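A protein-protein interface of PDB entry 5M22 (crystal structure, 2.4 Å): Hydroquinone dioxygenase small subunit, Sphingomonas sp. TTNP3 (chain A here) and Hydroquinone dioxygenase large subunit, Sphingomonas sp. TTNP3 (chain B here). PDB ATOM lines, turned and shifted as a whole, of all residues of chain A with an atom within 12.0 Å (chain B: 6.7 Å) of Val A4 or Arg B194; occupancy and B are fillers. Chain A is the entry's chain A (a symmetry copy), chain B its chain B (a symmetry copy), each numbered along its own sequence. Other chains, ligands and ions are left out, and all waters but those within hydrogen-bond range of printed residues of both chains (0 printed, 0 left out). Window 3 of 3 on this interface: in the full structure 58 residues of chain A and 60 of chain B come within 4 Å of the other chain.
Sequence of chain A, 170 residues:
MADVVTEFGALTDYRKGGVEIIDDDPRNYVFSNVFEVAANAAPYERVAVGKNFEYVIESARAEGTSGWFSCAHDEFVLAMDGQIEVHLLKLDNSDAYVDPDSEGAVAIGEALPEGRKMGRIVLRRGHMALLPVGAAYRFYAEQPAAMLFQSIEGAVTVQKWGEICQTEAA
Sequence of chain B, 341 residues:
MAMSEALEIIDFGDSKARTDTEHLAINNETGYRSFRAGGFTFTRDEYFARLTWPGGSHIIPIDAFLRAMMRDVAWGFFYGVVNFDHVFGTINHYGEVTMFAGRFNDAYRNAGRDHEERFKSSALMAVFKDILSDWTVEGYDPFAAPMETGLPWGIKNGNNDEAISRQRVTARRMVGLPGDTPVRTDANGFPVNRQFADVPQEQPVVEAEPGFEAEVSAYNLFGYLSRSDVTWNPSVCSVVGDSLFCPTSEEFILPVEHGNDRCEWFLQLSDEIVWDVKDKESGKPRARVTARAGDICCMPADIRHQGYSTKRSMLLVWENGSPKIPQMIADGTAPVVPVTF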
ATOM      1  N   ASP A   3     -17.517 -12.823   5.179  1.00  0.00           N
ATOM      2  CA  ASP A   3     -17.555 -11.474   4.579  1.00  0.00           C
ATOM      3  C   ASP A   3     -18.984 -10.986   4.352  1.00  0.00           C
ATOM      4  O   ASP A   3     -19.517 -11.055   3.236  1.00  0.00           O
ATOM      5  CB  ASP A   3     -16.768 -11.477   3.273  1.00  0.00           C
ATOM      6  CG  ASP A   3     -15.481 -10.694   3.383  1.00  0.00           C
ATOM      7  OD1 ASP A   3     -15.275 -10.051   4.443  1.00  0.00           O
ATOM      8  OD2 ASP A   3     -14.683 -10.719   2.412  1.00  0.00           O
ATOM      9  N   VAL A   4     -19.595 -10.478   5.412  1.00  0.00           N
ATOM     10  CA  VAL A   4     -21.001 -10.055   5.387  1.00  0.00           C
ATOM     11  C   VAL A   4     -21.277  -8.844   4.463  1.00  0.00           C
ATOM     12  O   VAL A   4     -20.628  -7.806   4.579  1.00  0.00           O
ATOM     13  CB  VAL A   4     -21.484  -9.785   6.827  1.00  0.00           C
ATOM     14  CG1 VAL A   4     -22.999  -9.627   6.877  1.00  0.00           C
ATOM     15  CG2 VAL A   4     -21.064 -10.935   7.731  1.00  0.00           C
ATOM     16  N   VAL A   5     -22.222  -8.991   3.530  1.00  0.00           N
ATOM     17  CA  VAL A   5     -22.692  -7.826   2.748  1.00  0.00           C
ATOM     18  C   VAL A   5     -24.153  -7.526   3.042  1.00  0.00           C
ATOM     19  O   VAL A   5     -25.044  -8.335   2.741  1.00  0.00           O
ATOM     20  CB  VAL A   5     -22.506  -7.961   1.205  1.00  0.00           C
ATOM     21  CG1 VAL A   5     -22.486  -6.583   0.558  1.00  0.00           C
ATOM     22  CG2 VAL A   5     -21.220  -8.701   0.860  1.00  0.00           C
ATOM     23  N   THR A   6     -24.392  -6.361   3.632  1.00  0.00           N
ATOM     24  CA  THR A   6     -25.749  -5.900   3.805  1.00  0.00           C
ATOM     25  C   THR A   6     -26.204  -5.025   2.626  1.00  0.00           C
ATOM     26  O   THR A   6     -25.784  -3.876   2.452  1.00  0.00           O
ATOM     27  CB  THR A   6     -25.964  -5.254   5.191  1.00  0.00           C
ATOM     28  OG1 THR A   6     -25.486  -6.150   6.195  1.00  0.00           O
ATOM     29  CG2 THR A   6     -27.422  -5.021   5.432  1.00  0.00           C
ATOM     30  N   GLU A   7     -27.068  -5.607   1.811  1.00  0.00           N
ATOM     31  CA  GLU A   7     -27.581  -4.978   0.605  1.00  0.00           C
ATOM     32  C   GLU A   7     -28.462  -3.759   0.927  1.00  0.00           C
ATOM     33  O   GLU A   7     -29.451  -3.896   1.638  1.00  0.00           O
ATOM     34  CB  GLU A   7     -28.406  -6.021  -0.146  1.00  0.00           C
ATOM     35  CG  GLU A   7     -28.297  -5.926  -1.652  1.00  0.00           C
ATOM     36  CD  GLU A   7     -26.873  -6.131  -2.147  1.00  0.00           C
ATOM     37  OE1 GLU A   7     -26.225  -7.124  -1.757  1.00  0.00           O
ATOM     38  OE2 GLU A   7     -26.410  -5.292  -2.946  1.00  0.00           O
ATOM     39  N   PHE A   8     -28.104  -2.578   0.424  1.00  0.00           N
ATOM     40  CA  PHE A   8     -29.004  -1.412   0.481  1.00  0.00           C
ATOM     41  C   PHE A   8     -29.321  -0.889  -0.926  1.00  0.00           C
ATOM     42  O   PHE A   8     -28.508  -1.009  -1.860  1.00  0.00           O
ATOM     43  CB  PHE A   8     -28.412  -0.286   1.326  1.00  0.00           C
ATOM     44  CG  PHE A   8     -28.323  -0.597   2.808  1.00  0.00           C
ATOM     45  CD1 PHE A   8     -29.467  -0.582   3.623  1.00  0.00           C
ATOM     46  CD2 PHE A   8     -27.070  -0.870   3.415  1.00  0.00           C
ATOM     47  CE1 PHE A   8     -29.359  -0.857   4.994  1.00  0.00           C
ATOM     48  CE2 PHE A   8     -26.964  -1.142   4.786  1.00  0.00           C
ATOM     49  CZ  PHE A   8     -28.114  -1.136   5.576  1.00  0.00           C
ATOM     50  N   ARG A 125     -27.461   8.089   4.152  1.00  0.00           N
ATOM     51  CA  ARG A 125     -28.335   6.896   4.121  1.00  0.00           C
ATOM     52  C   ARG A 125     -28.587   6.307   5.535  1.00  0.00           C
ATOM     53  O   ARG A 125     -27.651   6.115   6.316  1.00  0.00           O
ATOM     54  CB  ARG A 125     -27.774   5.819   3.171  1.00  0.00           C
ATOM     55  CG  ARG A 125     -28.573   4.523   3.115  1.00  0.00           C
ATOM     56  CD  ARG A 125     -27.850   3.450   2.337  1.00  0.00           C
ATOM     57  NE  ARG A 125     -26.723   2.954   3.105  1.00  0.00           N
ATOM     58  CZ  ARG A 125     -25.693   2.291   2.583  1.00  0.00           C
ATOM     59  NH1 ARG A 125     -25.654   2.034   1.278  1.00  0.00           N
ATOM     60  NH2 ARG A 125     -24.696   1.888   3.371  1.00  0.00           N
ATOM     61  N   ALA B 145     -32.572 -15.958  16.176  1.00  0.00           N
ATOM     62  CA  ALA B 145     -32.521 -16.922  15.037  1.00  0.00           C
ATOM     63  C   ALA B 145     -31.877 -18.261  15.440  1.00  0.00           C
ATOM     64  O   ALA B 145     -31.084 -18.286  16.384  1.00  0.00           O
ATOM     65  CB  ALA B 145     -31.756 -16.310  13.873  1.00  0.00           C
ATOM     66  N   PRO B 146     -32.181 -19.377  14.728  1.00  0.00           N
ATOM     67  CA  PRO B 146     -31.566 -20.661  15.209  1.00  0.00           C
ATOM     68  C   PRO B 146     -30.025 -20.692  15.183  1.00  0.00           C
ATOM     69  O   PRO B 146     -29.407 -21.355  16.017  1.00  0.00           O
ATOM     70  CB  PRO B 146     -32.147 -21.709  14.286  1.00  0.00           C
ATOM     71  CG  PRO B 146     -33.403 -21.110  13.756  1.00  0.00           C
ATOM     72  CD  PRO B 146     -33.257 -19.614  13.747  1.00  0.00           C
ATOM     73  N   MET B 147     -29.399 -19.958  14.274  1.00  0.00           N
ATOM     74  CA  MET B 147     -27.944 -19.905  14.252  1.00  0.00           C
ATOM     75  C   MET B 147     -27.314 -19.173  15.436  1.00  0.00           C
ATOM     76  O   MET B 147     -26.142 -19.316  15.685  1.00  0.00           O
ATOM     77  CB  MET B 147     -27.426 -19.363  12.916  1.00  0.00           C
ATOM     78  CG  MET B 147     -27.640 -20.388  11.801  1.00  0.00           C
ATOM     79  SD  MET B 147     -26.680 -20.152  10.298  1.00  0.00           S
ATOM     80  CE  MET B 147     -25.118 -20.871  10.789  1.00  0.00           C
ATOM     81  N   GLU B 148     -28.103 -18.417  16.177  1.00  0.00           N
ATOM     82  CA  GLU B 148     -27.584 -17.550  17.225  1.00  0.00           C
ATOM     83  C   GLU B 148     -27.684 -18.124  18.640  1.00  0.00           C
ATOM     84  O   GLU B 148     -27.187 -17.520  19.567  1.00  0.00           O
ATOM     85  CB  GLU B 148     -28.402 -16.269  17.255  1.00  0.00           C
ATOM     86  CG  GLU B 148     -28.541 -15.533  15.952  1.00  0.00           C
ATOM     87  CD  GLU B 148     -29.151 -14.176  16.185  1.00  0.00           C
ATOM     88  OE1 GLU B 148     -30.379 -14.074  16.240  1.00  0.00           O
ATOM     89  OE2 GLU B 148     -28.383 -13.214  16.341  1.00  0.00           O
ATOM     90  N   PRO B 191     -24.303  -4.197  20.991  1.00  0.00           N
ATOM     91  CA  PRO B 191     -23.340  -4.125  19.915  1.00  0.00           C
ATOM     92  C   PRO B 191     -23.988  -4.589  18.594  1.00  0.00           C
ATOM     93  O   PRO B 191     -25.070  -5.166  18.599  1.00  0.00           O
ATOM     94  CB  PRO B 191     -22.236  -5.089  20.392  1.00  0.00           C
ATOM     95  CG  PRO B 191     -22.976  -6.142  21.131  1.00  0.00           C
ATOM     96  CD  PRO B 191     -24.172  -5.447  21.766  1.00  0.00           C
ATOM     97  N   VAL B 192     -23.314  -4.330  17.484  1.00  0.00           N
ATOM     98  CA  VAL B 192     -23.779  -4.672  16.135  1.00  0.00           C
ATOM     99  C   VAL B 192     -23.853  -6.193  15.965  1.00  0.00           C
ATOM    100  O   VAL B 192     -22.948  -6.905  16.368  1.00  0.00           O
ATOM    101  CB  VAL B 192     -22.816  -4.045  15.105  1.00  0.00           C
ATOM    102  CG1 VAL B 192     -23.146  -4.461  13.689  1.00  0.00           C
ATOM    103  CG2 VAL B 192     -22.876  -2.538  15.214  1.00  0.00           C
ATOM    104  N   ASN B 193     -24.938  -6.680  15.384  1.00  0.00           N
ATOM    105  CA  ASN B 193     -25.098  -8.101  15.130  1.00  0.00           C
ATOM    106  C   ASN B 193     -24.086  -8.596  14.063  1.00  0.00           C
ATOM    107  O   ASN B 193     -23.754  -7.836  13.152  1.00  0.00           O
ATOM    108  CB  ASN B 193     -26.526  -8.338  14.644  1.00  0.00           C
ATOM    109  CG  ASN B 193     -26.841  -9.803  14.486  1.00  0.00           C
ATOM    110  OD1 ASN B 193     -26.527 -10.426  13.464  1.00  0.00           O
ATOM    111  ND2 ASN B 193     -27.461 -10.364  15.497  1.00  0.00           N
ATOM    112  N   ARG B 194     -23.599  -9.840  14.161  1.00  0.00           N
ATOM    113  CA  ARG B 194     -22.580 -10.317  13.208  1.00  0.00           C
ATOM    114  C   ARG B 194     -23.027 -10.175  11.741  1.00  0.00           C
ATOM    115  O   ARG B 194     -22.208  -9.960  10.851  1.00  0.00           O
ATOM    116  CB  ARG B 194     -22.137 -11.772  13.507  1.00  0.00           C
ATOM    117  CG  ARG B 194     -23.041 -12.906  12.994  1.00  0.00           C
ATOM    118  CD  ARG B 194     -24.326 -13.073  13.813  1.00  0.00           C
ATOM    119  NE  ARG B 194     -25.079 -14.274  13.445  1.00  0.00           N
ATOM    120  CZ  ARG B 194     -26.369 -14.321  13.075  1.00  0.00           C
ATOM    121  NH1 ARG B 194     -26.918 -15.490  12.775  1.00  0.00           N
ATOM    122  NH2 ARG B 194     -27.123 -13.230  13.005  1.00  0.00           N
ATOM    123  N   GLN B 195     -24.330 -10.280  11.496  1.00  0.00           N
ATOM    124  CA  GLN B 195     -24.860 -10.246  10.141  1.00  0.00           C
ATOM    125  C   GLN B 195     -25.260  -8.847   9.617  1.00  0.00           C
ATOM    126  O   GLN B 195     -25.945  -8.714   8.600  1.00  0.00           O
ATOM    127  CB  GLN B 195     -26.015 -11.227  10.031  1.00  0.00           C
ATOM    128  CG  GLN B 195     -25.529 -12.656  10.060  1.00  0.00           C
ATOM    129  CD  GLN B 195     -26.419 -13.597   9.308  1.00  0.00           C
ATOM    130  OE1 GLN B 195     -27.567 -13.280   8.981  1.00  0.00           O
ATOM    131  NE2 GLN B 195     -25.909 -14.793   9.055  1.00  0.00           N
ATOM    132  N   PHE B 196     -24.798  -7.833  10.332  1.00  0.00           N
ATOM    133  CA  PHE B 196     -24.881  -6.439   9.948  1.00  0.00           C
ATOM    134  C   PHE B 196     -23.517  -5.765  10.218  1.00  0.00           C
ATOM    135  O   PHE B 196     -23.472  -4.553  10.509  1.00  0.00           O
ATOM    136  CB  PHE B 196     -25.939  -5.746  10.806  1.00  0.00           C
ATOM    137  CG  PHE B 196     -27.351  -6.045  10.408  1.00  0.00           C
ATOM    138  CD1 PHE B 196     -27.759  -5.935   9.064  1.00  0.00           C
ATOM    139  CD2 PHE B 196     -28.304  -6.358  11.383  1.00  0.00           C
ATOM    140  CE1 PHE B 196     -29.083  -6.190   8.708  1.00  0.00           C
ATOM    141  CE2 PHE B 196     -29.631  -6.588  11.040  1.00  0.00           C
ATOM    142  CZ  PHE B 196     -30.021  -6.511   9.704  1.00  0.00           C
ATOM    143  N   ALA B 197     -22.421  -6.529  10.189  1.00  0.00           N
ATOM    144  CA  ALA B 197     -21.108  -5.969  10.592  1.00  0.00           C
ATOM    145  C   ALA B 197     -20.592  -4.845   9.665  1.00  0.00           C
ATOM    146  O   ALA B 197     -19.831  -3.984  10.093  1.00  0.00           O
ATOM    147  CB  ALA B 197     -20.050  -7.067  10.732  1.00  0.00           C
ATOM    148  N   ASP B 198     -21.015  -4.866   8.406  1.00  0.00           N
ATOM    149  CA  ASP B 198     -20.629  -3.846   7.455  1.00  0.00           C
ATOM    150  C   ASP B 198     -21.454  -2.537   7.538  1.00  0.00           C
ATOM    151  O   ASP B 198     -21.119  -1.551   6.870  1.00  0.00           O
ATOM    152  CB  ASP B 198     -20.636  -4.416   6.029  1.00  0.00           C
ATOM    153  CG  ASP B 198     -22.023  -4.857   5.559  1.00  0.00           C
ATOM    154  OD1 ASP B 198     -22.854  -5.325   6.364  1.00  0.00           O
ATOM    155  OD2 ASP B 198     -22.270  -4.753   4.342  1.00  0.00           O
ATOM    156  N   SER B 226     -29.314  -2.402  13.356  1.00  0.00           N
ATOM    157  CA  SER B 226     -28.205  -3.352  13.271  1.00  0.00           C
ATOM    158  C   SER B 226     -27.798  -3.809  14.636  1.00  0.00           C
ATOM    159  O   SER B 226     -27.083  -4.810  14.783  1.00  0.00           O
ATOM    160  CB  SER B 226     -26.971  -2.714  12.642  1.00  0.00           C
ATOM    161  OG  SER B 226     -26.302  -1.897  13.593  1.00  0.00           O
ATOM    162  N   GLU B 251     -34.765 -12.468  10.802  1.00  0.00           N
ATOM    163  CA  GLU B 251     -33.892 -13.598  10.449  1.00  0.00           C
ATOM    164  C   GLU B 251     -34.658 -14.903  10.598  1.00  0.00           C
ATOM    165  O   GLU B 251     -35.468 -15.055  11.500  1.00  0.00           O
ATOM    166  CB  GLU B 251     -32.613 -13.612  11.305  1.00  0.00           C
ATOM    167  CG  GLU B 251     -31.465 -14.408  10.681  1.00  0.00           C
ATOM    168  CD  GLU B 251     -30.214 -14.473  11.552  1.00  0.00           C
ATOM    169  OE1 GLU B 251     -29.874 -13.459  12.226  1.00  0.00           O
ATOM    170  OE2 GLU B 251     -29.552 -15.542  11.539  1.00  0.00           O
ATOM    171  N   LYS B 311     -30.657 -13.979   5.222  1.00  0.00           N
ATOM    172  CA  LYS B 311     -29.729 -13.135   5.947  1.00  0.00           C
ATOM    173  C   LYS B 311     -30.554 -12.249   6.863  1.00  0.00           C
ATOM    174  O   LYS B 311     -31.712 -11.940   6.583  1.00  0.00           O
ATOM    175  CB  LYS B 311     -28.942 -12.262   4.972  1.00  0.00           C
ATOM    176  CG  LYS B 311     -27.851 -11.458   5.648  1.00  0.00           C
ATOM    177  CD  LYS B 311     -27.341 -10.365   4.742  1.00  0.00           C
ATOM    178  CE  LYS B 311     -26.543  -9.371   5.547  1.00  0.00           C
ATOM    179  NZ  LYS B 311     -27.384  -8.236   6.021  1.00  0.00           N
ATOM    180  N   ARG B 312     -29.943 -11.822   7.948  1.00  0.00           N
ATOM    181  CA  ARG B 312     -30.617 -10.977   8.880  1.00  0.00           C
ATOM    182  C   ARG B 312     -30.855  -9.706   8.094  1.00  0.00           C
ATOM    183  O   ARG B 312     -29.922  -9.153   7.505  1.00  0.00           O
ATOM    184  CB  ARG B 312     -29.752 -10.724  10.109  1.00  0.00           C
ATOM    185  CG  ARG B 312     -30.454  -9.962  11.230  1.00  0.00           C
ATOM    186  CD  ARG B 312     -29.534  -9.854  12.427  1.00  0.00           C
ATOM    187  NE  ARG B 312     -30.157  -9.487  13.697  1.00  0.00           N
ATOM    188  CZ  ARG B 312     -30.532 -10.368  14.629  1.00  0.00           C
ATOM    189  NH1 ARG B 312     -30.398 -11.682  14.428  1.00  0.00           N
ATOM    190  NH2 ARG B 312     -31.055  -9.936  15.765  1.00  0.00           N
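Arg B194 touches Val A4.
Val A4 touches Gln B195.
Lys B311 touches Val A4 (CE to CG1, 3.8 Å).
Val A5 touches Asp B198.
Val A5 touches Lys B311 (O to CE, 3.3 Å).
Thr A6 touches Gln B195 (OG1 to O, 3.5 Å).
Phe B196 touches Thr A6.
The side-chain hydroxyl (OG1) of Thr A6 sits at hydrogen-bond distance from the side-chain amino group (NZ) of Lys B311.
N of Thr A6 lies within hydrogen-bond range of OD2 of Asp B198.
O of Val A4 sits close to OD2 of Asp B198.
Of the 16 printed residues of chain B, 5 touch a printed residue of chain A.
Along chain B the printed residues that touch a printed residue of chain A span positions 194 to 311.
Printed residues of chain A that touch a printed residue of chain B: Val A4, Val A5 and Thr A6.
Hydrophobic or aromatic side chains of chain A within 4 Å of the printed part of chain B: Val A4.
Among the printed residues, no Asp or Glu carboxylate lies within 4 Å of a Lys or Arg side-chain nitrogen of the other chain.
NH2 of Arg B194 lies within salt-bridge range of OE1 of Glu B251.
The side-chain amino group of Lys B311 is in hydrogen-bond range of the backbone carbonyl oxygen of Gln B195 (3.0 Å).
OE2 of Glu B148 is in salt-bridge range of NH2 of Arg B194, at 3.6 Å.
The backbone NH of Gln B195 is in hydrogen-bond range of the side-chain amide oxygen of Asn B193 (3.0 Å).
The side-chain amide oxygen (OD1) of Asn B193 sits at hydrogen-bond distance from the guanidinium group (NH2) of Arg B194.
OE1 of Gln B195 lies within hydrogen-bond range of N of Arg B312, 3.0 Å away.
Printed residues of chain B within 4 Å of Thr A6: Gln B195 (3.5 Å), Phe B196 (3.7 Å), Asp B198 (2.8 Å) and Lys B311 (2.8 Å).
No residue of chain A comes within 4 Å of Ala B145.
Pro B191 touches none of the printed residues of chain A.
No residue of chain A comes within 4 Å of Val B192.
No residue of chain A comes within 4 Å of Asn B193.
Of chain A, only Val A4 (3.5 Å) comes within 4 Å of Arg B194.
Of chain A, only Val A4 (3.5 Å) and Thr A6 (3.5 Å) come within 4 Å of Gln B195.
Of the printed residues of chain A, Phe B196 touches Thr A6 (3.7 Å).
Of the printed residues of chain A, Lys B311 touches Val A4, Val A5 and Thr A6.
No residue of chain A comes within 4 Å of Arg B312.
The nearest residue of chain B that does not touch Val A4 is Phe B196 (4.3 Å).
The nearest residue of chain A that does not touch Arg B194 is Thr A6 (6.9 Å).
The nearest printed residue of chain B that does not touch Thr A6 is Ala B197 (5.0 Å).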
